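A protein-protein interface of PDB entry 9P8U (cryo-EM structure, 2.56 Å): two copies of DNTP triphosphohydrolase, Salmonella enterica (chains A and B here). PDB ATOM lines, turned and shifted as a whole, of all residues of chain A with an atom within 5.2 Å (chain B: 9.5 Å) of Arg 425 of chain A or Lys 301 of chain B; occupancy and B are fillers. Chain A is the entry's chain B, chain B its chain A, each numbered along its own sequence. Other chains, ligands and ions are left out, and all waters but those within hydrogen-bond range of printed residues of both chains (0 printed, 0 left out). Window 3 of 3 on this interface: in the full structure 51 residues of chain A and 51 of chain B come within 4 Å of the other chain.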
ATOM      1  N   ILE A 175     -18.252  33.135  20.344  1.00  0.00           N
ATOM      2  CA  ILE A 175     -18.988  31.876  20.264  1.00  0.00           C
ATOM      3  C   ILE A 175     -20.456  32.098  20.603  1.00  0.00           C
ATOM      4  O   ILE A 175     -21.354  31.573  19.933  1.00  0.00           O
ATOM      5  CB  ILE A 175     -18.346  30.820  21.179  1.00  0.00           C
ATOM      6  CG1 ILE A 175     -16.988  30.387  20.620  1.00  0.00           C
ATOM      7  CG2 ILE A 175     -19.271  29.623  21.335  1.00  0.00           C
ATOM      8  CD1 ILE A 175     -16.502  29.054  21.145  1.00  0.00           C
ATOM      9  N   LEU A 176     -20.725  32.885  21.639  1.00  0.00           N
ATOM     10  CA  LEU A 176     -22.096  33.195  22.019  1.00  0.00           C
ATOM     11  C   LEU A 176     -22.635  34.293  21.111  1.00  0.00           C
ATOM     12  O   LEU A 176     -22.135  35.423  21.130  1.00  0.00           O
ATOM     13  CB  LEU A 176     -22.160  33.619  23.483  1.00  0.00           C
ATOM     14  CG  LEU A 176     -23.543  33.566  24.129  1.00  0.00           C
ATOM     15  CD1 LEU A 176     -23.990  32.125  24.293  1.00  0.00           C
ATOM     16  CD2 LEU A 176     -23.534  34.284  25.467  1.00  0.00           C
ATOM     17  N   ASN A 177     -23.650  33.964  20.317  1.00  0.00           N
ATOM     18  CA  ASN A 177     -24.237  34.911  19.370  1.00  0.00           C
ATOM     19  C   ASN A 177     -25.214  35.807  20.117  1.00  0.00           C
ATOM     20  O   ASN A 177     -26.389  35.480  20.292  1.00  0.00           O
ATOM     21  CB  ASN A 177     -24.924  34.175  18.226  1.00  0.00           C
ATOM     22  CG  ASN A 177     -25.425  35.114  17.146  1.00  0.00           C
ATOM     23  OD1 ASN A 177     -25.165  36.316  17.182  1.00  0.00           O
ATOM     24  ND2 ASN A 177     -26.154  34.568  16.181  1.00  0.00           N
ATOM     25  N   GLU A 421     -18.567  26.975  14.084  1.00  0.00           N
ATOM     26  CA  GLU A 421     -20.005  27.017  14.329  1.00  0.00           C
ATOM     27  C   GLU A 421     -20.512  28.432  14.569  1.00  0.00           C
ATOM     28  O   GLU A 421     -21.643  28.745  14.190  1.00  0.00           O
ATOM     29  CB  GLU A 421     -20.364  26.122  15.514  1.00  0.00           C
ATOM     30  CG  GLU A 421     -20.447  24.646  15.173  1.00  0.00           C
ATOM     31  CD  GLU A 421     -19.084  23.990  15.075  1.00  0.00           C
ATOM     32  OE1 GLU A 421     -18.081  24.641  15.430  1.00  0.00           O
ATOM     33  OE2 GLU A 421     -19.016  22.821  14.640  1.00  0.00           O
ATOM     34  N   ASN A 422     -19.717  29.290  15.212  1.00  0.00           N
ATOM     35  CA  ASN A 422     -20.183  30.647  15.486  1.00  0.00           C
ATOM     36  C   ASN A 422     -20.383  31.437  14.197  1.00  0.00           C
ATOM     37  O   ASN A 422     -21.363  32.182  14.066  1.00  0.00           O
ATOM     38  CB  ASN A 422     -19.206  31.366  16.414  1.00  0.00           C
ATOM     39  CG  ASN A 422     -17.778  31.276  15.935  1.00  0.00           C
ATOM     40  OD1 ASN A 422     -17.397  30.317  15.269  1.00  0.00           O
ATOM     41  ND2 ASN A 422     -16.977  32.278  16.271  1.00  0.00           N
ATOM     42  N   TYR A 423     -19.468  31.289  13.238  1.00  0.00           N
ATOM     43  CA  TYR A 423     -19.620  31.981  11.963  1.00  0.00           C
ATOM     44  C   TYR A 423     -20.872  31.516  11.234  1.00  0.00           C
ATOM     45  O   TYR A 423     -21.619  32.332  10.681  1.00  0.00           O
ATOM     46  CB  TYR A 423     -18.385  31.761  11.092  1.00  0.00           C
ATOM     47  CG  TYR A 423     -17.084  32.163  11.745  1.00  0.00           C
ATOM     48  CD1 TYR A 423     -17.029  33.225  12.633  1.00  0.00           C
ATOM     49  CD2 TYR A 423     -15.909  31.477  11.470  1.00  0.00           C
ATOM     50  CE1 TYR A 423     -15.842  33.592  13.231  1.00  0.00           C
ATOM     51  CE2 TYR A 423     -14.719  31.838  12.063  1.00  0.00           C
ATOM     52  CZ  TYR A 423     -14.691  32.896  12.942  1.00  0.00           C
ATOM     53  OH  TYR A 423     -13.506  33.260  13.535  1.00  0.00           O
ATOM     54  N   ARG A 424     -21.123  30.205  11.226  1.00  0.00           N
ATOM     55  CA  ARG A 424     -22.324  29.684  10.584  1.00  0.00           C
ATOM     56  C   ARG A 424     -23.581  30.150  11.303  1.00  0.00           C
ATOM     57  O   ARG A 424     -24.603  30.424  10.664  1.00  0.00           O
ATOM     58  CB  ARG A 424     -22.270  28.161  10.531  1.00  0.00           C
ATOM     59  CG  ARG A 424     -21.345  27.619   9.465  1.00  0.00           C
ATOM     60  CD  ARG A 424     -21.496  26.120   9.328  1.00  0.00           C
ATOM     61  NE  ARG A 424     -20.694  25.398  10.305  1.00  0.00           N
ATOM     62  CZ  ARG A 424     -21.158  24.435  11.089  1.00  0.00           C
ATOM     63  NH1 ARG A 424     -22.425  24.058  11.042  1.00  0.00           N
ATOM     64  NH2 ARG A 424     -20.332  23.836  11.940  1.00  0.00           N
ATOM     65  N   ARG A 425     -23.532  30.229  12.632  1.00  0.00           N
ATOM     66  CA  ARG A 425     -24.675  30.711  13.398  1.00  0.00           C
ATOM     67  C   ARG A 425     -24.983  32.161  13.058  1.00  0.00           C
ATOM     68  O   ARG A 425     -26.149  32.545  12.909  1.00  0.00           O
ATOM     69  CB  ARG A 425     -24.399  30.552  14.891  1.00  0.00           C
ATOM     70  CG  ARG A 425     -25.585  30.835  15.786  1.00  0.00           C
ATOM     71  CD  ARG A 425     -25.243  30.523  17.228  1.00  0.00           C
ATOM     72  NE  ARG A 425     -24.658  29.194  17.362  1.00  0.00           N
ATOM     73  CZ  ARG A 425     -23.423  28.958  17.779  1.00  0.00           C
ATOM     74  NH1 ARG A 425     -22.609  29.943  18.122  1.00  0.00           N
ATOM     75  NH2 ARG A 425     -22.992  27.703  17.854  1.00  0.00           N
ATOM     76  N   ILE A 426     -23.943  32.987  12.940  1.00  0.00           N
ATOM     77  CA  ILE A 426     -24.140  34.375  12.535  1.00  0.00           C
ATOM     78  C   ILE A 426     -24.707  34.440  11.124  1.00  0.00           C
ATOM     79  O   ILE A 426     -25.627  35.217  10.841  1.00  0.00           O
ATOM     80  CB  ILE A 426     -22.819  35.157  12.651  1.00  0.00           C
ATOM     81  CG1 ILE A 426     -22.490  35.432  14.119  1.00  0.00           C
ATOM     82  CG2 ILE A 426     -22.895  36.454  11.867  1.00  0.00           C
ATOM     83  CD1 ILE A 426     -23.127  36.690  14.666  1.00  0.00           C
ATOM     84  N   PHE A 427     -24.173  33.619  10.218  1.00  0.00           N
ATOM     85  CA  PHE A 427     -24.607  33.651   8.826  1.00  0.00           C
ATOM     86  C   PHE A 427     -26.065  33.233   8.682  1.00  0.00           C
ATOM     87  O   PHE A 427     -26.812  33.824   7.895  1.00  0.00           O
ATOM     88  CB  PHE A 427     -23.702  32.752   7.984  1.00  0.00           C
ATOM     89  CG  PHE A 427     -24.293  32.356   6.667  1.00  0.00           C
ATOM     90  CD1 PHE A 427     -24.331  33.249   5.612  1.00  0.00           C
ATOM     91  CD2 PHE A 427     -24.802  31.085   6.478  1.00  0.00           C
ATOM     92  CE1 PHE A 427     -24.871  32.884   4.398  1.00  0.00           C
ATOM     93  CE2 PHE A 427     -25.343  30.716   5.268  1.00  0.00           C
ATOM     94  CZ  PHE A 427     -25.379  31.616   4.227  1.00  0.00           C
ATOM     95  N   GLU A 428     -26.489  32.214   9.428  1.00  0.00           N
ATOM     96  CA  GLU A 428     -27.849  31.705   9.322  1.00  0.00           C
ATOM     97  C   GLU A 428     -28.869  32.562  10.058  1.00  0.00           C
ATOM     98  O   GLU A 428     -30.071  32.386   9.837  1.00  0.00           O
ATOM     99  CB  GLU A 428     -27.916  30.272   9.852  1.00  0.00           C
ATOM    100  CG  GLU A 428     -27.192  29.259   8.989  1.00  0.00           C
ATOM    101  CD  GLU A 428     -26.828  28.003   9.752  1.00  0.00           C
ATOM    102  OE1 GLU A 428     -27.167  27.917  10.950  1.00  0.00           O
ATOM    103  OE2 GLU A 428     -26.203  27.102   9.155  1.00  0.00           O
ATOM    104  N   GLN A 429     -28.426  33.469  10.923  1.00  0.00           N
ATOM    105  CA  GLN A 429     -29.357  34.327  11.643  1.00  0.00           C
ATOM    106  C   GLN A 429     -30.087  35.250  10.677  1.00  0.00           C
ATOM    107  O   GLN A 429     -29.506  35.755   9.713  1.00  0.00           O
ATOM    108  CB  GLN A 429     -28.611  35.147  12.694  1.00  0.00           C
ATOM    109  CG  GLN A 429     -29.507  35.996  13.573  1.00  0.00           C
ATOM    110  CD  GLN A 429     -28.734  37.040  14.348  1.00  0.00           C
ATOM    111  OE1 GLN A 429     -27.526  37.190  14.172  1.00  0.00           O
ATOM    112  NE2 GLN A 429     -29.428  37.769  15.214  1.00  0.00           N
ATOM    113  N   ALA B 295     -26.814  26.489  32.704  1.00  0.00           N
ATOM    114  CA  ALA B 295     -28.227  26.352  32.364  1.00  0.00           C
ATOM    115  C   ALA B 295     -28.626  27.349  31.280  1.00  0.00           C
ATOM    116  O   ALA B 295     -29.246  26.980  30.272  1.00  0.00           O
ATOM    117  CB  ALA B 295     -29.088  26.536  33.614  1.00  0.00           C
ATOM    118  N   ASP B 296     -28.253  28.618  31.460  1.00  0.00           N
ATOM    119  CA  ASP B 296     -28.590  29.641  30.476  1.00  0.00           C
ATOM    120  C   ASP B 296     -27.920  29.363  29.138  1.00  0.00           C
ATOM    121  O   ASP B 296     -28.522  29.575  28.079  1.00  0.00           O
ATOM    122  CB  ASP B 296     -28.193  31.021  30.997  1.00  0.00           C
ATOM    123  CG  ASP B 296     -28.814  31.333  32.341  1.00  0.00           C
ATOM    124  OD1 ASP B 296     -29.134  30.380  33.082  1.00  0.00           O
ATOM    125  OD2 ASP B 296     -28.981  32.529  32.657  1.00  0.00           O
ATOM    126  N   TYR B 297     -26.670  28.899  29.160  1.00  0.00           N
ATOM    127  CA  TYR B 297     -25.989  28.571  27.912  1.00  0.00           C
ATOM    128  C   TYR B 297     -26.666  27.401  27.208  1.00  0.00           C
ATOM    129  O   TYR B 297     -26.784  27.384  25.978  1.00  0.00           O
ATOM    130  CB  TYR B 297     -24.517  28.275  28.182  1.00  0.00           C
ATOM    131  CG  TYR B 297     -23.732  29.514  28.526  1.00  0.00           C
ATOM    132  CD1 TYR B 297     -24.100  30.750  28.015  1.00  0.00           C
ATOM    133  CD2 TYR B 297     -22.635  29.455  29.372  1.00  0.00           C
ATOM    134  CE1 TYR B 297     -23.392  31.891  28.326  1.00  0.00           C
ATOM    135  CE2 TYR B 297     -21.924  30.591  29.692  1.00  0.00           C
ATOM    136  CZ  TYR B 297     -22.304  31.806  29.164  1.00  0.00           C
ATOM    137  OH  TYR B 297     -21.597  32.943  29.479  1.00  0.00           O
ATOM    138  N   ALA B 298     -27.119  26.409  27.978  1.00  0.00           N
ATOM    139  CA  ALA B 298     -27.853  25.293  27.393  1.00  0.00           C
ATOM    140  C   ALA B 298     -29.189  25.743  26.821  1.00  0.00           C
ATOM    141  O   ALA B 298     -29.712  25.110  25.898  1.00  0.00           O
ATOM    142  CB  ALA B 298     -28.063  24.197  28.437  1.00  0.00           C
ATOM    143  N   GLN B 299     -29.759  26.826  27.356  1.00  0.00           N
ATOM    144  CA  GLN B 299     -30.976  27.373  26.763  1.00  0.00           C
ATOM    145  C   GLN B 299     -30.737  27.818  25.324  1.00  0.00           C
ATOM    146  O   GLN B 299     -31.596  27.625  24.456  1.00  0.00           O
ATOM    147  CB  GLN B 299     -31.506  28.533  27.604  1.00  0.00           C
ATOM    148  CG  GLN B 299     -31.917  28.140  29.011  1.00  0.00           C
ATOM    149  CD  GLN B 299     -32.698  26.841  29.045  1.00  0.00           C
ATOM    150  OE1 GLN B 299     -33.747  26.718  28.412  1.00  0.00           O
ATOM    151  NE2 GLN B 299     -32.190  25.864  29.785  1.00  0.00           N
ATOM    152  N   GLN B 300     -29.579  28.415  25.051  1.00  0.00           N
ATOM    153  CA  GLN B 300     -29.237  28.792  23.689  1.00  0.00           C
ATOM    154  C   GLN B 300     -28.904  27.552  22.863  1.00  0.00           C
ATOM    155  O   GLN B 300     -28.890  26.422  23.357  1.00  0.00           O
ATOM    156  CB  GLN B 300     -28.057  29.763  23.676  1.00  0.00           C
ATOM    157  CG  GLN B 300     -27.995  30.700  24.869  1.00  0.00           C
ATOM    158  CD  GLN B 300     -29.219  31.583  24.981  1.00  0.00           C
ATOM    159  OE1 GLN B 300     -29.544  32.332  24.061  1.00  0.00           O
ATOM    160  NE2 GLN B 300     -29.909  31.499  26.112  1.00  0.00           N
ATOM    161  N   LYS B 301     -28.628  27.775  21.580  1.00  0.00           N
ATOM    162  CA  LYS B 301     -28.248  26.706  20.663  1.00  0.00           C
ATOM    163  C   LYS B 301     -26.732  26.733  20.491  1.00  0.00           C
ATOM    164  O   LYS B 301     -26.162  27.740  20.059  1.00  0.00           O
ATOM    165  CB  LYS B 301     -28.980  26.844  19.327  1.00  0.00           C
ATOM    166  CG  LYS B 301     -28.689  28.119  18.540  1.00  0.00           C
ATOM    167  CD  LYS B 301     -29.875  28.536  17.684  1.00  0.00           C
ATOM    168  CE  LYS B 301     -31.158  28.614  18.498  1.00  0.00           C
ATOM    169  NZ  LYS B 301     -30.981  29.394  19.755  1.00  0.00           N
ATOM    170  N   LEU B 302     -26.079  25.633  20.857  1.00  0.00           N
ATOM    171  CA  LEU B 302     -24.629  25.533  20.785  1.00  0.00           C
ATOM    172  C   LEU B 302     -24.232  24.087  20.541  1.00  0.00           C
ATOM    173  O   LEU B 302     -24.910  23.163  20.997  1.00  0.00           O
ATOM    174  CB  LEU B 302     -23.962  26.038  22.073  1.00  0.00           C
ATOM    175  CG  LEU B 302     -23.632  27.526  22.191  1.00  0.00           C
ATOM    176  CD1 LEU B 302     -24.757  28.281  22.875  1.00  0.00           C
ATOM    177  CD2 LEU B 302     -22.328  27.723  22.940  1.00  0.00           C
ATOM    178  N   SER B 303     -23.127  23.898  19.822  1.00  0.00           N
ATOM    179  CA  SER B 303     -22.570  22.570  19.652  1.00  0.00           C
ATOM    180  C   SER B 303     -21.991  22.088  20.981  1.00  0.00           C
ATOM    181  O   SER B 303     -21.664  22.898  21.852  1.00  0.00           O
ATOM    182  CB  SER B 303     -21.493  22.579  18.570  1.00  0.00           C
ATOM    183  OG  SER B 303     -20.315  23.217  19.027  1.00  0.00           O
ATOM    184  N   PRO B 304     -21.877  20.769  21.169  1.00  0.00           N
ATOM    185  CA  PRO B 304     -21.313  20.270  22.435  1.00  0.00           C
ATOM    186  C   PRO B 304     -19.927  20.812  22.730  1.00  0.00           C
ATOM    187  O   PRO B 304     -19.627  21.143  23.885  1.00  0.00           O
ATOM    188  CB  PRO B 304     -21.298  18.749  22.230  1.00  0.00           C
ATOM    189  CG  PRO B 304     -22.366  18.497  21.226  1.00  0.00           C
ATOM    190  CD  PRO B 304     -22.340  19.673  20.301  1.00  0.00           C
ATOM    191  N   ALA B 305     -19.075  20.931  21.710  1.00  0.00           N
ATOM    192  CA  ALA B 305     -17.754  21.512  21.919  1.00  0.00           C
ATOM    193  C   ALA B 305     -17.855  22.975  22.324  1.00  0.00           C
ATOM    194  O   ALA B 305     -17.125  23.434  23.209  1.00  0.00           O
ATOM    195  CB  ALA B 305     -16.905  21.359  20.659  1.00  0.00           C
ATOM    196  N   GLU B 306     -18.757  23.724  21.689  1.00  0.00           N
ATOM    197  CA  GLU B 306     -18.925  25.132  22.032  1.00  0.00           C
ATOM    198  C   GLU B 306     -19.481  25.298  23.442  1.00  0.00           C
ATOM    199  O   GLU B 306     -19.063  26.199  24.179  1.00  0.00           O
ATOM    200  CB  GLU B 306     -19.828  25.813  21.008  1.00  0.00           C
ATOM    201  CG  GLU B 306     -19.097  26.265  19.757  1.00  0.00           C
ATOM    202  CD  GLU B 306     -19.922  27.210  18.910  1.00  0.00           C
ATOM    203  OE1 GLU B 306     -21.147  27.286  19.129  1.00  0.00           O
ATOM    204  OE2 GLU B 306     -19.342  27.879  18.029  1.00  0.00           O
ATOM    205  N   LEU B 307     -20.434  24.447  23.829  1.00  0.00           N
ATOM    206  CA  LEU B 307     -20.951  24.487  25.192  1.00  0.00           C
ATOM    207  C   LEU B 307     -19.854  24.174  26.199  1.00  0.00           C
ATOM    208  O   LEU B 307     -19.743  24.833  27.239  1.00  0.00           O
ATOM    209  CB  LEU B 307     -22.114  23.509  25.343  1.00  0.00           C
ATOM    210  CG  LEU B 307     -23.136  23.849  26.427  1.00  0.00           C
ATOM    211  CD1 LEU B 307     -23.697  25.243  26.212  1.00  0.00           C
ATOM    212  CD2 LEU B 307     -24.250  22.819  26.450  1.00  0.00           C
ATOM    213  N   MET B 310     -17.568  27.301  26.424  1.00  0.00           N
ATOM    214  CA  MET B 310     -18.163  28.394  27.189  1.00  0.00           C
ATOM    215  C   MET B 310     -18.219  28.081  28.678  1.00  0.00           C
ATOM    216  O   MET B 310     -17.932  28.943  29.519  1.00  0.00           O
ATOM    217  CB  MET B 310     -19.557  28.720  26.648  1.00  0.00           C
ATOM    218  CG  MET B 310     -20.014  30.155  26.905  1.00  0.00           C
ATOM    219  SD  MET B 310     -19.256  31.505  25.975  1.00  0.00           S
ATOM    220  CE  MET B 310     -18.424  30.650  24.647  1.00  0.00           C
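The backbone carbonyl oxygen (O) of Lys 301 of chain B is in hydrogen-bond range of the guanidinium group (NE) of Arg 425 of chain A (3.4 Å).
The backbone NH of Asn 422 of chain A sits at hydrogen-bond distance from the side-chain carboxylate of Glu 306 of chain B.
The side-chain carboxylate of Glu 306 of chain B lies within salt-bridge range of the guanidinium group of Arg 425 of chain A, at 3.2 Å.
No position is printed for both chains.
Of the 9 pairs that touch across the chains among the printed residues, none has its exchanged pair printed and touching as well.
Hydrophobic or aromatic side chains of chain A within 4 Å of the printed part of chain B: Ile 175 and Leu 176.
Of the 14 printed residues of chain B, 5 touch a printed residue of chain A.
Hydrophobic or aromatic side chains of chain B within 4 Å of the printed part of chain A: Tyr 297, Leu 302 and Met 310.
Among the printed residues, Asp or Glu carboxylates within 4 Å of a Lys or Arg side-chain nitrogen of the other chain: Arg 425 of chain A with Glu 306 of chain B (2.3 Å).
Lys 301 of chain B touches just one residue of chain A: Arg 425 (3.4 Å).
No residue of chain B comes within 4 Å of Ile 426 of chain A.
No residue of chain B comes within 4 Å of Glu 428 of chain A.
Of the printed residues of chain A, Tyr 297 of chain B touches Leu 176.
Printed residues of chain B within 4 Å of Ile 175 of chain A: Leu 302, Glu 306 and Met 310.
Gln 299 of chain B touches none of the printed residues of chain A.
Ala 305 of chain B touches none of the printed residues of chain A.
The nearest printed residue of chain A that does not touch Tyr 297 of chain B is Ile 175 of chain A (8.3 Å).
OG of Ser 303 of chain B lies within hydrogen-bond range of N of Glu 306 of chain B (3.1 Å).
The guanidinium group (NH1) of Arg 425 of chain A is in hydrogen-bond range of the backbone carbonyl oxygen (O) of Ile 175 of chain A, at 2.7 Å.
The side-chain carboxylate (OE2) of Glu 421 of chain A lies within salt-bridge range of the guanidinium group (NH2) of Arg 424 of chain A (3.2 Å).
Leu 302 of chain B touches Ile 175 of chain A (CD2 to CG2, 3.9 Å).
Ile 175 of chain A touches Glu 306 of chain B.
Ile 175 of chain A touches Met 310 of chain B (CB to CE, 3.5 Å).
Tyr 297 of chain B touches Leu 176 of chain A (CE1 to CD2, 3.7 Å).
Glu 306 of chain B touches Glu 421 of chain A (OE2 to CB, 3.2 Å).
Leu 302 of chain B touches Arg 425 of chain A.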
